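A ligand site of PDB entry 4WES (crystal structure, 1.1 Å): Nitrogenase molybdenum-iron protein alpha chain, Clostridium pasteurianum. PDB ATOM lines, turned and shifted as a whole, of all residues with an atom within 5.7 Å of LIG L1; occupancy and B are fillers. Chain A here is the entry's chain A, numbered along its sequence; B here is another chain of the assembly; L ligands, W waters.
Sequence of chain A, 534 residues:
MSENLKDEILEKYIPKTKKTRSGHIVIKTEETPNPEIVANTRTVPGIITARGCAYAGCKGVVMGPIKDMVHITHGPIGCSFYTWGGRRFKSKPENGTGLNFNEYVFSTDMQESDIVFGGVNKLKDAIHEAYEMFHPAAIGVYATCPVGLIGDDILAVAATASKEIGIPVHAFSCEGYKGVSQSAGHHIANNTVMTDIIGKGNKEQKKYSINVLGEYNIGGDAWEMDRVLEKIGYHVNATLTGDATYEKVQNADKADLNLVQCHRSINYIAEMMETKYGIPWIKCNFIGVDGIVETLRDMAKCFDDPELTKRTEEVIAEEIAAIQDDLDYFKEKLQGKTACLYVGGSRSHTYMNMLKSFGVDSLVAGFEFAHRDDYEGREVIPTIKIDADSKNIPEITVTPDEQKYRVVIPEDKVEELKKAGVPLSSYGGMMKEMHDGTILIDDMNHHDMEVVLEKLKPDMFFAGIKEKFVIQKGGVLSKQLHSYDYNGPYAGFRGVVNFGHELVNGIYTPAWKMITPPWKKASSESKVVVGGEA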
ATOM      1  N   ALA A  50     -25.934  -2.398  24.871  1.00  0.00           N
ATOM      2  CA  ALA A  50     -24.515  -2.178  25.117  1.00  0.00           C
ATOM      3  C   ALA A  50     -24.237  -1.420  26.425  1.00  0.00           C
ATOM      4  O   ALA A  50     -23.104  -1.314  26.833  1.00  0.00           O
ATOM      5  CB  ALA A  50     -23.889  -1.421  23.961  1.00  0.00           C
ATOM      6  N   GLY A  52     -23.862   0.147  30.225  1.00  0.00           N
ATOM      7  CA  GLY A  52     -23.373  -0.211  31.550  1.00  0.00           C
ATOM      8  C   GLY A  52     -24.138   0.468  32.645  1.00  0.00           C
ATOM      9  O   GLY A  52     -25.299   0.838  32.475  1.00  0.00           O
ATOM     10  N   ALA A  56     -19.918   2.345  36.696  1.00  0.00           N
ATOM     11  CA  ALA A  56     -18.997   2.533  35.577  1.00  0.00           C
ATOM     12  C   ALA A  56     -18.852   4.012  35.263  1.00  0.00           C
ATOM     13  O   ALA A  56     -17.753   4.526  35.118  1.00  0.00           O
ATOM     14  CB  ALA A  56     -19.487   1.751  34.363  1.00  0.00           C
ATOM     15  N   GLY A  57     -19.984   4.718  35.161  1.00  0.00           N
ATOM     16  CA  GLY A  57     -19.934   6.127  34.805  1.00  0.00           C
ATOM     17  C   GLY A  57     -19.218   7.004  35.824  1.00  0.00           C
ATOM     18  O   GLY A  57     -18.584   8.008  35.488  1.00  0.00           O
ATOM     19  N   VAL A  61     -15.254   5.900  34.776  1.00  0.00           N
ATOM     20  CA  VAL A  61     -15.199   6.928  33.746  1.00  0.00           C
ATOM     21  C   VAL A  61     -14.701   8.261  34.307  1.00  0.00           C
ATOM     22  O   VAL A  61     -13.590   8.682  34.004  1.00  0.00           O
ATOM     23  CB  VAL A  61     -16.554   7.053  32.993  1.00  0.00           C
ATOM     24  CG1 VAL A  61     -16.546   8.247  32.057  1.00  0.00           C
ATOM     25  CG2 VAL A  61     -16.842   5.740  32.256  1.00  0.00           C
ATOM     26  N   GLY A  86      -9.093  -1.605  31.477  1.00  0.00           N
ATOM     27  CA  GLY A  86      -9.839  -1.758  30.236  1.00  0.00           C
ATOM     28  C   GLY A  86     -10.188  -0.445  29.567  1.00  0.00           C
ATOM     29  O   GLY A  86     -10.370  -0.391  28.353  1.00  0.00           O
ATOM     30  N   ARG A  87     -10.328   0.624  30.353  1.00  0.00           N
ATOM     31  CA  ARG A  87     -10.555   1.965  29.823  1.00  0.00           C
ATOM     32  C   ARG A  87      -9.197   2.680  29.865  1.00  0.00           C
ATOM     33  O   ARG A  87      -8.573   2.795  30.913  1.00  0.00           O
ATOM     34  CB  ARG A  87     -11.610   2.710  30.611  1.00  0.00           C
ATOM     35  CG  ARG A  87     -11.856   4.114  30.084  1.00  0.00           C
ATOM     36  CD  ARG A  87     -13.139   4.671  30.566  1.00  0.00           C
ATOM     37  NE  ARG A  87     -13.339   6.074  30.247  1.00  0.00           N
ATOM     38  CZ  ARG A  87     -12.977   7.101  31.025  1.00  0.00           C
ATOM     39  NH1 ARG A  87     -13.291   8.337  30.677  1.00  0.00           N
ATOM     40  NH2 ARG A  87     -12.305   6.897  32.161  1.00  0.00           N
ATOM     41  N   ARG A  88      -8.761   3.130  28.683  1.00  0.00           N
ATOM     42  CA  ARG A  88      -7.377   3.467  28.420  1.00  0.00           C
ATOM     43  C   ARG A  88      -7.014   4.934  28.686  1.00  0.00           C
ATOM     44  O   ARG A  88      -6.277   5.542  27.912  1.00  0.00           O
ATOM     45  CB  ARG A  88      -7.038   3.067  26.994  1.00  0.00           C
ATOM     46  CG  ARG A  88      -7.155   1.576  26.734  1.00  0.00           C
ATOM     47  CD  ARG A  88      -6.949   1.232  25.274  1.00  0.00           C
ATOM     48  NE  ARG A  88      -5.642   1.686  24.829  1.00  0.00           N
ATOM     49  CZ  ARG A  88      -5.366   2.705  23.998  1.00  0.00           C
ATOM     50  NH1 ARG A  88      -4.104   3.095  23.844  1.00  0.00           N
ATOM     51  NH2 ARG A  88      -6.317   3.338  23.346  1.00  0.00           N
ATOM     52  N   GLN A 182     -24.675   4.483  32.351  1.00  0.00           N
ATOM     53  CA  GLN A 182     -23.491   5.203  32.844  1.00  0.00           C
ATOM     54  C   GLN A 182     -23.781   6.658  33.182  1.00  0.00           C
ATOM     55  O   GLN A 182     -23.064   7.254  34.011  1.00  0.00           O
ATOM     56  CB  GLN A 182     -22.369   5.143  31.812  1.00  0.00           C
ATOM     57  CG  GLN A 182     -21.791   3.763  31.501  1.00  0.00           C
ATOM     58  CD  GLN A 182     -22.450   3.111  30.290  1.00  0.00           C
ATOM     59  OE1 GLN A 182     -23.659   3.027  30.222  1.00  0.00           O
ATOM     60  NE2 GLN A 182     -21.648   2.570  29.395  1.00  0.00           N
ATOM     61  N   GLU A 368     -25.470   5.147  23.316  1.00  0.00           N
ATOM     62  CA  GLU A 368     -25.980   4.282  24.378  1.00  0.00           C
ATOM     63  C   GLU A 368     -26.860   5.039  25.346  1.00  0.00           C
ATOM     64  O   GLU A 368     -27.912   4.516  25.748  1.00  0.00           O
ATOM     65  CB  GLU A 368     -24.838   3.637  25.157  1.00  0.00           C
ATOM     66  CG  GLU A 368     -23.941   2.659  24.424  1.00  0.00           C
ATOM     67  CD  GLU A 368     -22.857   2.061  25.311  1.00  0.00           C
ATOM     68  OE1 GLU A 368     -21.875   1.484  24.707  1.00  0.00           O
ATOM     69  OE2 GLU A 368     -22.942   2.120  26.558  1.00  0.00           O
ATOM     70  N   PHE A 369     -26.399   6.206  25.810  1.00  0.00           N
ATOM     71  CA  PHE A 369     -26.988   6.773  27.038  1.00  0.00           C
ATOM     72  C   PHE A 369     -27.057   8.289  27.041  1.00  0.00           C
ATOM     73  O   PHE A 369     -27.341   8.897  28.072  1.00  0.00           O
ATOM     74  CB  PHE A 369     -26.180   6.272  28.271  1.00  0.00           C
ATOM     75  CG  PHE A 369     -24.694   6.540  28.161  1.00  0.00           C
ATOM     76  CD1 PHE A 369     -24.172   7.826  28.228  1.00  0.00           C
ATOM     77  CD2 PHE A 369     -23.827   5.482  27.963  1.00  0.00           C
ATOM     78  CE1 PHE A 369     -22.861   8.056  28.027  1.00  0.00           C
ATOM     79  CE2 PHE A 369     -22.475   5.709  27.793  1.00  0.00           C
ATOM     80  CZ  PHE A 369     -21.997   6.992  27.784  1.00  0.00           C
ATOM     81  N   ALA A 463     -17.988   1.110  16.773  1.00  0.00           N
ATOM     82  CA  ALA A 463     -18.740   0.808  17.988  1.00  0.00           C
ATOM     83  C   ALA A 463     -17.772   0.484  19.129  1.00  0.00           C
ATOM     84  O   ALA A 463     -16.747   1.197  19.273  1.00  0.00           O
ATOM     85  CB  ALA A 463     -19.796  -0.275  17.717  1.00  0.00           C
ATOM     86  N   GLY A 464     -18.053  -0.524  19.920  1.00  0.00           N
ATOM     87  CA  GLY A 464     -17.211  -0.942  21.001  1.00  0.00           C
ATOM     88  C   GLY A 464     -16.826  -2.397  20.916  1.00  0.00           C
ATOM     89  O   GLY A 464     -17.030  -3.060  19.851  1.00  0.00           O
ATOM     90  N   ILE A 465     -16.334  -2.932  22.025  1.00  0.00           N
ATOM     91  CA  ILE A 465     -15.807  -4.273  22.047  1.00  0.00           C
ATOM     92  C   ILE A 465     -16.892  -5.359  21.925  1.00  0.00           C
ATOM     93  O   ILE A 465     -16.618  -6.445  21.427  1.00  0.00           O
ATOM     94  CB  ILE A 465     -14.949  -4.456  23.319  1.00  0.00           C
ATOM     95  CG1 ILE A 465     -14.134  -5.730  23.300  1.00  0.00           C
ATOM     96  CG2 ILE A 465     -15.798  -4.377  24.587  1.00  0.00           C
ATOM     97  CD1 ILE A 465     -13.175  -5.841  22.187  1.00  0.00           C
ATOM     98  N   LYS A 466     -18.090  -5.083  22.442  1.00  0.00           N
ATOM     99  CA  LYS A 466     -19.150  -6.090  22.396  1.00  0.00           C
ATOM    100  C   LYS A 466     -19.707  -6.230  20.996  1.00  0.00           C
ATOM    101  O   LYS A 466     -20.111  -7.336  20.607  1.00  0.00           O
ATOM    102  CB  LYS A 466     -20.252  -5.802  23.404  1.00  0.00           C
ATOM    103  CG  LYS A 466     -19.726  -5.750  24.844  1.00  0.00           C
ATOM    104  CD  LYS A 466     -20.814  -5.656  25.903  1.00  0.00           C
ATOM    105  CE  LYS A 466     -21.749  -4.488  25.799  1.00  0.00           C
ATOM    106  NZ  LYS A 466     -21.068  -3.166  25.871  1.00  0.00           N
ATOM    107  N   GLU A 467     -19.738  -5.160  20.223  1.00  0.00           N
ATOM    108  CA  GLU A 467     -20.231  -5.199  18.863  1.00  0.00           C
ATOM    109  C   GLU A 467     -19.175  -5.599  17.862  1.00  0.00           C
ATOM    110  O   GLU A 467     -19.499  -6.153  16.796  1.00  0.00           O
ATOM    111  CB  GLU A 467     -20.795  -3.842  18.460  1.00  0.00           C
ATOM    112  CG  GLU A 467     -21.880  -3.254  19.359  1.00  0.00           C
ATOM    113  CD  GLU A 467     -21.380  -2.324  20.455  1.00  0.00           C
ATOM    114  OE1 GLU A 467     -20.169  -2.394  20.822  1.00  0.00           O
ATOM    115  OE2 GLU A 467     -22.212  -1.496  20.935  1.00  0.00           O
ATOM    116  N   GLN A 480     -13.154   0.243  16.890  1.00  0.00           N
ATOM    117  CA  GLN A 480     -13.655   0.652  18.191  1.00  0.00           C
ATOM    118  C   GLN A 480     -13.405   2.151  18.451  1.00  0.00           C
ATOM    119  O   GLN A 480     -12.266   2.625  18.408  1.00  0.00           O
ATOM    120  CB  GLN A 480     -12.927  -0.124  19.276  1.00  0.00           C
ATOM    121  CG  GLN A 480     -13.143  -1.625  19.217  1.00  0.00           C
ATOM    122  CD  GLN A 480     -12.462  -2.317  20.365  1.00  0.00           C
ATOM    123  OE1 GLN A 480     -12.860  -2.172  21.542  1.00  0.00           O
ATOM    124  NE2 GLN A 480     -11.385  -3.049  20.093  1.00  0.00           N
ATOM    125  N   HIS A 482     -14.310   3.544  21.418  1.00  0.00           N
ATOM    126  CA  HIS A 482     -14.018   3.711  22.837  1.00  0.00           C
ATOM    127  C   HIS A 482     -12.522   3.476  23.081  1.00  0.00           C
ATOM    128  O   HIS A 482     -11.770   4.381  23.470  1.00  0.00           O
ATOM    129  CB  HIS A 482     -14.818   2.774  23.755  1.00  0.00           C
ATOM    130  CG  HIS A 482     -16.301   2.737  23.601  1.00  0.00           C
ATOM    131  ND1 HIS A 482     -17.171   3.165  24.586  1.00  0.00           N
ATOM    132  CD2 HIS A 482     -17.064   2.148  22.633  1.00  0.00           C
ATOM    133  CE1 HIS A 482     -18.398   2.818  24.232  1.00  0.00           C
ATOM    134  NE2 HIS A 482     -18.357   2.219  23.049  1.00  0.00           N
ATOM    135  N   SER A 483     -12.074   2.249  22.841  1.00  0.00           N
ATOM    136  CA  SER A 483     -10.711   1.845  23.117  1.00  0.00           C
ATOM    137  C   SER A 483      -9.706   2.185  22.041  1.00  0.00           C
ATOM    138  O   SER A 483      -8.490   1.974  22.216  1.00  0.00           O
ATOM    139  CB  SER A 483     -10.615   0.347  23.329  1.00  0.00           C
ATOM    140  OG  SER A 483     -10.793  -0.318  22.069  1.00  0.00           O
ATOM    141  N   SER B  50     -22.628  -6.306  30.855  1.00  0.00           N
ATOM    142  CA  SER B  50     -21.692  -5.668  29.931  1.00  0.00           C
ATOM    143  C   SER B  50     -20.240  -5.996  30.245  1.00  0.00           C
ATOM    144  O   SER B  50     -19.470  -6.375  29.359  1.00  0.00           O
ATOM    145  CB  SER B  50     -21.875  -4.150  29.926  1.00  0.00           C
ATOM    146  OG  SER B  50     -21.026  -3.571  28.924  1.00  0.00           O
ATOM    147  N   TYR B  51     -19.867  -5.880  31.523  1.00  0.00           N
ATOM    148  CA  TYR B  51     -18.503  -6.199  31.909  1.00  0.00           C
ATOM    149  C   TYR B  51     -18.131  -7.645  31.629  1.00  0.00           C
ATOM    150  O   TYR B  51     -17.018  -7.963  31.216  1.00  0.00           O
ATOM    151  CB  TYR B  51     -18.279  -5.883  33.382  1.00  0.00           C
ATOM    152  CG  TYR B  51     -18.066  -4.450  33.776  1.00  0.00           C
ATOM    153  CD1 TYR B  51     -17.519  -3.491  32.918  1.00  0.00           C
ATOM    154  CD2 TYR B  51     -18.265  -4.067  35.099  1.00  0.00           C
ATOM    155  CE1 TYR B  51     -17.216  -2.213  33.349  1.00  0.00           C
ATOM    156  CE2 TYR B  51     -17.973  -2.779  35.535  1.00  0.00           C
ATOM    157  CZ  TYR B  51     -17.433  -1.870  34.679  1.00  0.00           C
ATOM    158  OH  TYR B  51     -17.150  -0.606  35.153  1.00  0.00           O
ATOM    159  N   THR B  54     -17.804  -8.449  28.048  1.00  0.00           N
ATOM    160  CA  THR B  54     -16.606  -7.778  27.570  1.00  0.00           C
ATOM    161  C   THR B  54     -15.361  -8.563  27.822  1.00  0.00           C
ATOM    162  O   THR B  54     -14.479  -8.655  26.944  1.00  0.00           O
ATOM    163  CB  THR B  54     -16.536  -6.355  28.178  1.00  0.00           C
ATOM    164  OG1 THR B  54     -17.594  -5.564  27.618  1.00  0.00           O
ATOM    165  CG2 THR B  54     -15.217  -5.677  27.915  1.00  0.00           C
ATOM    166  N   ARG B  58     -12.617  -9.824  25.106  1.00  0.00           N
ATOM    167  CA  ARG B  58     -11.205  -9.429  25.170  1.00  0.00           C
ATOM    168  C   ARG B  58     -10.244 -10.614  25.200  1.00  0.00           C
ATOM    169  O   ARG B  58      -9.126 -10.533  24.683  1.00  0.00           O
ATOM    170  CB  ARG B  58     -10.965  -8.520  26.397  1.00  0.00           C
ATOM    171  CG  ARG B  58     -11.583  -7.169  26.249  1.00  0.00           C
ATOM    172  CD  ARG B  58     -11.504  -6.365  27.565  1.00  0.00           C
ATOM    173  NE  ARG B  58     -11.903  -4.972  27.342  1.00  0.00           N
ATOM    174  CZ  ARG B  58     -12.292  -4.146  28.318  1.00  0.00           C
ATOM    175  NH1 ARG B  58     -12.224  -4.539  29.598  1.00  0.00           N
ATOM    176  NH2 ARG B  58     -12.730  -2.946  28.005  1.00  0.00           N
HETATM  177  C1  LIG L   1     -17.887   1.695  30.116  1.00  0.00           C
HETATM  178  C2  LIG L   1     -16.446   1.731  29.591  1.00  0.00           C
HETATM  179  C3  LIG L   1     -16.336   1.712  28.064  1.00  0.00           C
HETATM  180  C4  LIG L   1     -16.507   0.287  27.490  1.00  0.00           C
HETATM  181  C5  LIG L   1     -16.121   0.324  26.002  1.00  0.00           C
HETATM  182  C6  LIG L   1     -16.608  -0.759  25.092  1.00  0.00           C
HETATM  183  C7  LIG L   1     -14.962   2.221  27.655  1.00  0.00           C
HETATM  184  O1  LIG L   1     -18.812   2.079  29.390  1.00  0.00           O
HETATM  185  O2  LIG L   1     -18.062   1.308  31.281  1.00  0.00           O
HETATM  186  O3  LIG L   1     -15.806  -1.201  24.208  1.00  0.00           O
HETATM  187  O4  LIG L   1     -17.769  -1.192  25.215  1.00  0.00           O
HETATM  188  O5  LIG L   1     -14.910   3.141  26.811  1.00  0.00           O
HETATM  189  O6  LIG L   1     -13.952   1.667  28.120  1.00  0.00           O
HETATM  190  O7  LIG L   1     -17.340   2.535  27.483  1.00  0.00           O
HETATM  191 FE1  LG2 L   2     -17.914  11.191  27.427  1.00  0.00          FE
HETATM  192 MO1  LG2 L   2     -16.711   4.407  26.504  1.00  0.00          MO
HETATM  193 FE2  LG2 L   2     -18.446   8.750  28.350  1.00  0.00          FE
HETATM  194 FE3  LG2 L   2     -16.015   9.318  27.403  1.00  0.00          FE
HETATM  195 FE4  LG2 L   2     -18.091   9.192  25.756  1.00  0.00          FE
HETATM  196 FE5  LG2 L   2     -17.674   6.668  25.413  1.00  0.00          FE
HETATM  197 FE6  LG2 L   2     -17.962   6.246  27.996  1.00  0.00          FE
HETATM  198 FE7  LG2 L   2     -15.619   6.791  27.040  1.00  0.00          FE
HETATM  199  C1  LG2 L   2     -17.323   7.869  26.959  1.00  0.00           C
HETATM  200  S1  LG2 L   2     -19.833   9.975  27.045  1.00  0.00           S
HETATM  201  S2  LG2 L   2     -18.949   5.075  26.376  1.00  0.00           S
HETATM  202  S3  LG2 L   2     -16.989  10.247  29.252  1.00  0.00           S
HETATM  203  S4  LG2 L   2     -19.179   7.079  29.615  1.00  0.00           S
HETATM  204  S5  LG2 L   2     -18.554   8.076  23.886  1.00  0.00           S
HETATM  205  S6  LG2 L   2     -16.078   5.258  28.615  1.00  0.00           S
HETATM  206  S7  LG2 L   2     -16.434  10.776  25.714  1.00  0.00           S
HETATM  207  S8  LG2 L   2     -15.632   5.864  25.023  1.00  0.00           S
HETATM  208  S9  LG2 L   2     -14.050   8.256  27.508  1.00  0.00           S
HETATM  209  O   HOH W   1     -20.126   0.145  26.128  1.00  0.00           O
HETATM  210  O   HOH W   2     -13.211  -1.713  25.302  1.00  0.00           O
HETATM  211  O   HOH W   3     -13.618  -0.660  29.729  1.00  0.00           O
HETATM  212  O   HOH W   4     -19.427  -2.613  23.534  1.00  0.00           O
HETATM  213  O   HOH W   5     -14.169   0.047  22.330  1.00  0.00           O
HETATM  214  O   HOH W   6     -16.106   1.097  33.269  1.00  0.00           O
HETATM  215  O   HOH W   7     -12.590   4.825  26.741  1.00  0.00           O
HETATM  216  O   HOH W   8     -20.065  -0.553  31.318  1.00  0.00           O
HETATM  217  O   HOH W   9     -18.520  -3.002  27.145  1.00  0.00           O
HETATM  218  O   HOH W  10     -12.104   0.621  26.441  1.00  0.00           O
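O7 of LIG L1 lies close to ND1 of His 482 (3.0 Å). Residues that only touch LIG L1: Ala 56 (3.4 Å), Gly 464 (3.5 Å) and Arg 87 (3.6 Å). Of the 23 residues printed, 7 come within 4 Å of LIG L1.
The side-chain amide nitrogen (NE2) of Gln 182 lies within hydrogen-bond range of the side-chain carboxylate (OE2) of Glu 368 (3.2 Å). The side-chain amide oxygen (OE1) of Gln 182 lies within hydrogen-bond range of the backbone NH (N) of Gly 52 (2.9 Å). O of Ala 56 sits at hydrogen-bond distance from N of Val 61, 2.9 Å away. The backbone NH of Gly 464 sits at hydrogen-bond distance from the side-chain carboxylate of Glu 467, 3.0 Å away. O of Val 61 lies within hydrogen-bond range of NH2 of Arg 87 (2.9 Å). NZ of Lys 466 lies within hydrogen-bond range of OG of Ser 50 of chain B, at 3.1 Å. The side-chain amino group (NZ) of Lys 466 lies within hydrogen-bond range of the backbone carbonyl oxygen (O) of Ala 50 of chain A.
Water W10 lies within hydrogen-bond range of an oxygen (O6) of LIG L1 (2.7 Å) and the backbone carbonyl oxygen (O) of Gly 86 (2.8 Å). Water W9 lies within hydrogen-bond range of O4 of LIG L1 (2.8 Å), OG1 of Thr 54 of chain B (2.8 Å), NZ of Lys 466 (2.9 Å) and OG of Ser 50 of chain B (3.1 Å). Water W4 lies within hydrogen-bond range of an oxygen (O4) of LIG L1 (2.8 Å), the side-chain carboxylate (OE1) of Glu 467 (2.8 Å), the side-chain amino group (NZ) of Lys 466 (2.9 Å) and the backbone NH (N) of Ile 465 (3.5 Å). Water W6 lies within hydrogen-bond range of the side-chain hydroxyl of Tyr 51 of chain B (2.7 Å) and an oxygen (O2) of LIG L1 (2.8 Å). Water W3 lies within hydrogen-bond range of an oxygen (O6) of LIG L1 (2.8 Å) and the guanidinium group of Arg 58 of chain B (3.0 Å). Water W1 lies within hydrogen-bond range of the side-chain carboxylate (OE1) of Glu 368, an oxygen (O4) of LIG L1, the backbone carbonyl oxygen (O) of Ala 50 of chain A and the side-chain amino group (NZ) of Lys 466.
O7 of LIG L1 is bound to MO1 of LG2 L2 (2.2 Å).
N of Ile 465 is in hydrogen-bond range of O3 of LIG L1. NE2 of Gln 182 lies within hydrogen-bond range of O1 of LIG L1, 2.9 Å away. The side-chain amino group (NZ) of Lys 466 lies within salt-bridge range of an oxygen (O4) of LIG L1 (3.9 Å). A ring nitrogen (ND1) of His 482 is bound to a molybdenum atom (MO1) of LG2 L2 (2.3 Å). S9 of LG2 L2 sits close to NH1 of Arg 87 (3.3 Å).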
